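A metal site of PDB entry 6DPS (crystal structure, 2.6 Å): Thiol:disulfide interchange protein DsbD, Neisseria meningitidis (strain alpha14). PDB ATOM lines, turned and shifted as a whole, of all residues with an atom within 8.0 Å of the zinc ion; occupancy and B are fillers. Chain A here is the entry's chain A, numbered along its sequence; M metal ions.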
ATOM      1  N   GLY A  33       0.484  24.352   0.616  1.00  0.00           N
ATOM      2  CA  GLY A  33       1.610  24.163   1.519  1.00  0.00           C
ATOM      3  C   GLY A  33       2.312  22.818   1.401  1.00  0.00           C
ATOM      4  O   GLY A  33       3.184  22.520   2.240  1.00  0.00           O
ATOM      5  N   TYR A  34       1.956  22.001   0.402  1.00  0.00           N
ATOM      6  CA  TYR A  34       2.581  20.699   0.175  1.00  0.00           C
ATOM      7  C   TYR A  34       2.998  20.611  -1.282  1.00  0.00           C
ATOM      8  O   TYR A  34       2.585  21.432  -2.096  1.00  0.00           O
ATOM      9  CB  TYR A  34       1.617  19.555   0.570  1.00  0.00           C
ATOM     10  CG  TYR A  34       1.237  19.623   2.025  1.00  0.00           C
ATOM     11  CD1 TYR A  34       0.267  20.517   2.466  1.00  0.00           C
ATOM     12  CD2 TYR A  34       1.884  18.825   2.985  1.00  0.00           C
ATOM     13  CE1 TYR A  34      -0.057  20.608   3.803  1.00  0.00           C
ATOM     14  CE2 TYR A  34       1.555  18.914   4.330  1.00  0.00           C
ATOM     15  CZ  TYR A  34       0.570  19.812   4.737  1.00  0.00           C
ATOM     16  OH  TYR A  34       0.208  19.921   6.063  1.00  0.00           O
ATOM     17  N   TYR A  35       3.850  19.632  -1.599  1.00  0.00           N
ATOM     18  CA  TYR A  35       4.265  19.400  -2.984  1.00  0.00           C
ATOM     19  C   TYR A  35       4.696  17.962  -3.151  1.00  0.00           C
ATOM     20  O   TYR A  35       4.850  17.233  -2.169  1.00  0.00           O
ATOM     21  CB  TYR A  35       5.420  20.310  -3.410  1.00  0.00           C
ATOM     22  CG  TYR A  35       6.686  20.129  -2.641  1.00  0.00           C
ATOM     23  CD1 TYR A  35       6.899  20.813  -1.446  1.00  0.00           C
ATOM     24  CD2 TYR A  35       7.703  19.322  -3.132  1.00  0.00           C
ATOM     25  CE1 TYR A  35       8.084  20.685  -0.750  1.00  0.00           C
ATOM     26  CE2 TYR A  35       8.907  19.180  -2.438  1.00  0.00           C
ATOM     27  CZ  TYR A  35       9.079  19.871  -1.245  1.00  0.00           C
ATOM     28  OH  TYR A  35      10.246  19.760  -0.534  1.00  0.00           O
ATOM     29  N   MET A  36       4.869  17.540  -4.408  1.00  0.00           N
ATOM     30  CA  MET A  36       5.106  16.135  -4.732  1.00  0.00           C
ATOM     31  C   MET A  36       6.288  15.981  -5.681  1.00  0.00           C
ATOM     32  O   MET A  36       6.509  16.808  -6.564  1.00  0.00           O
ATOM     33  CB  MET A  36       3.869  15.477  -5.373  1.00  0.00           C
ATOM     34  CG  MET A  36       2.697  15.202  -4.434  1.00  0.00           C
ATOM     35  SD  MET A  36       1.323  14.494  -5.368  1.00  0.00           S
ATOM     36  CE  MET A  36       1.781  12.763  -5.259  1.00  0.00           C
ATOM     37  N   GLU A  60       7.115  21.934 -11.922  1.00  0.00           N
ATOM     38  CA  GLU A  60       8.145  22.941 -11.725  1.00  0.00           C
ATOM     39  C   GLU A  60       9.431  22.345 -11.154  1.00  0.00           C
ATOM     40  O   GLU A  60       9.450  21.241 -10.597  1.00  0.00           O
ATOM     41  CB  GLU A  60       7.698  24.067 -10.794  1.00  0.00           C
ATOM     42  CG  GLU A  60       6.412  24.693 -11.210  1.00  0.00           C
ATOM     43  CD  GLU A  60       5.274  24.146 -10.421  1.00  0.00           C
ATOM     44  OE1 GLU A  60       4.292  23.671 -11.020  1.00  0.00           O
ATOM     45  OE2 GLU A  60       5.388  24.177  -9.192  1.00  0.00           O
ATOM     46  N   GLU A  61      10.488  23.122 -11.289  1.00  0.00           N
ATOM     47  CA  GLU A  61      11.812  22.730 -10.865  1.00  0.00           C
ATOM     48  C   GLU A  61      12.075  23.366  -9.507  1.00  0.00           C
ATOM     49  O   GLU A  61      11.666  24.499  -9.256  1.00  0.00           O
ATOM     50  CB  GLU A  61      12.854  23.180 -11.890  1.00  0.00           C
ATOM     51  CG  GLU A  61      14.272  22.793 -11.572  1.00  0.00           C
ATOM     52  CD  GLU A  61      15.190  23.088 -12.738  1.00  0.00           C
ATOM     53  OE1 GLU A  61      16.002  24.030 -12.621  1.00  0.00           O
ATOM     54  OE2 GLU A  61      15.086  22.387 -13.760  1.00  0.00           O
ATOM     55  N   LYS A  62      12.690  22.605  -8.625  1.00  0.00           N
ATOM     56  CA  LYS A  62      12.910  23.109  -7.284  1.00  0.00           C
ATOM     57  C   LYS A  62      14.230  22.584  -6.775  1.00  0.00           C
ATOM     58  O   LYS A  62      14.575  21.410  -6.992  1.00  0.00           O
ATOM     59  CB  LYS A  62      11.780  22.712  -6.324  1.00  0.00           C
ATOM     60  CG  LYS A  62      12.167  22.761  -4.860  1.00  0.00           C
ATOM     61  CD  LYS A  62      11.078  22.183  -3.967  1.00  0.00           C
ATOM     62  CE  LYS A  62       9.798  23.004  -4.145  1.00  0.00           C
ATOM     63  NZ  LYS A  62       8.795  22.834  -3.066  1.00  0.00           N
ATOM     64  N   GLU A  63      14.968  23.446  -6.117  1.00  0.00           N
ATOM     65  CA  GLU A  63      16.128  23.040  -5.340  1.00  0.00           C
ATOM     66  C   GLU A  63      15.626  22.609  -3.965  1.00  0.00           C
ATOM     67  O   GLU A  63      15.081  23.419  -3.199  1.00  0.00           O
ATOM     68  CB  GLU A  63      17.162  24.170  -5.242  1.00  0.00           C
ATOM     69  CG  GLU A  63      18.240  23.974  -4.174  1.00  0.00           C
ATOM     70  CD  GLU A  63      18.934  22.604  -4.117  1.00  0.00           C
ATOM     71  OE1 GLU A  63      18.874  21.802  -5.113  1.00  0.00           O
ATOM     72  OE2 GLU A  63      19.594  22.362  -3.084  1.00  0.00           O
ATOM     73  N   ASP A  64      15.743  21.345  -3.678  1.00  0.00           N
ATOM     74  CA  ASP A  64      15.137  20.698  -2.540  1.00  0.00           C
ATOM     75  C   ASP A  64      16.217  20.266  -1.564  1.00  0.00           C
ATOM     76  O   ASP A  64      17.292  19.801  -1.939  1.00  0.00           O
ATOM     77  CB  ASP A  64      14.281  19.501  -3.021  1.00  0.00           C
ATOM     78  CG  ASP A  64      13.596  18.805  -1.910  1.00  0.00           C
ATOM     79  OD1 ASP A  64      14.200  17.864  -1.367  1.00  0.00           O
ATOM     80  OD2 ASP A  64      12.435  19.153  -1.606  1.00  0.00           O
ATOM     81  N   VAL A  72       8.875  19.071  -9.344  1.00  0.00           N
ATOM     82  CA  VAL A  72       7.891  18.874  -8.293  1.00  0.00           C
ATOM     83  C   VAL A  72       6.530  19.356  -8.764  1.00  0.00           C
ATOM     84  O   VAL A  72       6.389  19.926  -9.840  1.00  0.00           O
ATOM     85  CB  VAL A  72       8.276  19.559  -6.963  1.00  0.00           C
ATOM     86  CG1 VAL A  72       9.590  19.020  -6.473  1.00  0.00           C
ATOM     87  CG2 VAL A  72       8.364  21.057  -7.135  1.00  0.00           C
ATOM     88  N   TYR A  73       5.535  19.134  -7.925  1.00  0.00           N
ATOM     89  CA  TYR A  73       4.152  19.491  -8.223  1.00  0.00           C
ATOM     90  C   TYR A  73       3.524  20.232  -7.045  1.00  0.00           C
ATOM     91  O   TYR A  73       3.421  19.688  -5.940  1.00  0.00           O
ATOM     92  CB  TYR A  73       3.322  18.248  -8.545  1.00  0.00           C
ATOM     93  CG  TYR A  73       3.621  17.590  -9.867  1.00  0.00           C
ATOM     94  CD1 TYR A  73       3.291  18.218 -11.067  1.00  0.00           C
ATOM     95  CD2 TYR A  73       4.213  16.338  -9.923  1.00  0.00           C
ATOM     96  CE1 TYR A  73       3.563  17.610 -12.276  1.00  0.00           C
ATOM     97  CE2 TYR A  73       4.474  15.727 -11.115  1.00  0.00           C
ATOM     98  CZ  TYR A  73       4.153  16.359 -12.295  1.00  0.00           C
ATOM     99  OH  TYR A  73       4.429  15.743 -13.489  1.00  0.00           O
ATOM    100  N   HIS A  74       3.095  21.459  -7.288  1.00  0.00           N
ATOM    101  CA  HIS A  74       2.167  22.157  -6.418  1.00  0.00           C
ATOM    102  C   HIS A  74       0.746  22.075  -6.998  1.00  0.00           C
ATOM    103  O   HIS A  74       0.552  22.019  -8.214  1.00  0.00           O
ATOM    104  CB  HIS A  74       2.588  23.615  -6.250  1.00  0.00           C
ATOM    105  CG  HIS A  74       3.990  23.802  -5.763  1.00  0.00           C
ATOM    106  ND1 HIS A  74       5.039  24.116  -6.597  1.00  0.00           N
ATOM    107  CD2 HIS A  74       4.512  23.694  -4.517  1.00  0.00           C
ATOM    108  CE1 HIS A  74       6.154  24.209  -5.885  1.00  0.00           C
ATOM    109  NE2 HIS A  74       5.855  23.956  -4.618  1.00  0.00           N
ATOM    110  N   CYS A 100       5.849  16.260   0.238  1.00  0.00           N
ATOM    111  CA  CYS A 100       6.473  16.960   1.356  1.00  0.00           C
ATOM    112  C   CYS A 100       5.640  18.171   1.741  1.00  0.00           C
ATOM    113  O   CYS A 100       4.737  18.590   1.002  1.00  0.00           O
ATOM    114  CB  CYS A 100       7.916  17.422   1.016  1.00  0.00           C
ATOM    115  SG  CYS A 100       9.055  16.115   0.471  1.00  0.00           S
ATOM    116  N   ALA A 101       5.981  18.758   2.886  1.00  0.00           N
ATOM    117  CA  ALA A 101       5.413  20.027   3.310  1.00  0.00           C
ATOM    118  C   ALA A 101       6.427  21.142   3.068  1.00  0.00           C
ATOM    119  O   ALA A 101       7.617  20.961   3.325  1.00  0.00           O
ATOM    120  CB  ALA A 101       4.994  19.966   4.775  1.00  0.00           C
ATOM    121  N   GLU A 102       5.948  22.287   2.590  1.00  0.00           N
ATOM    122  CA  GLU A 102       6.805  23.457   2.371  1.00  0.00           C
ATOM    123  C   GLU A 102       7.505  23.927   3.638  1.00  0.00           C
ATOM    124  O   GLU A 102       8.547  24.586   3.545  1.00  0.00           O
ATOM    125  CB  GLU A 102       5.966  24.604   1.810  1.00  0.00           C
ATOM    126  CG  GLU A 102       5.281  24.253   0.501  1.00  0.00           C
ATOM    127  CD  GLU A 102       6.201  24.314  -0.707  1.00  0.00           C
ATOM    128  OE1 GLU A 102       7.417  24.516  -0.549  1.00  0.00           O
ATOM    129  OE2 GLU A 102       5.684  24.166  -1.822  1.00  0.00           O
HETATM  130 ZN    ZN M   1       7.259  24.409  -3.312  1.00  0.00          ZN
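The backbone NH of Glu 102 sits at hydrogen-bond distance from the backbone carbonyl oxygen of Gly 33 (2.8 Å).
ND1 of His 74 lies within hydrogen-bond range of OE2 of Glu 60, at 2.6 Å.
Three residues have an atom within 4 Å of the zinc ion: Lys 62, His 74 and Glu 102.
The zinc ion is bound by NE2 of His 74.
OE2 of Glu 102 is bound to the zinc ion.
The zinc ion is bound by NZ of Lys 62.
The zinc ion has three donor atoms within binding distance.
Slightly farther from the zinc ion lies OE1 of Glu 102 (2.8 Å).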
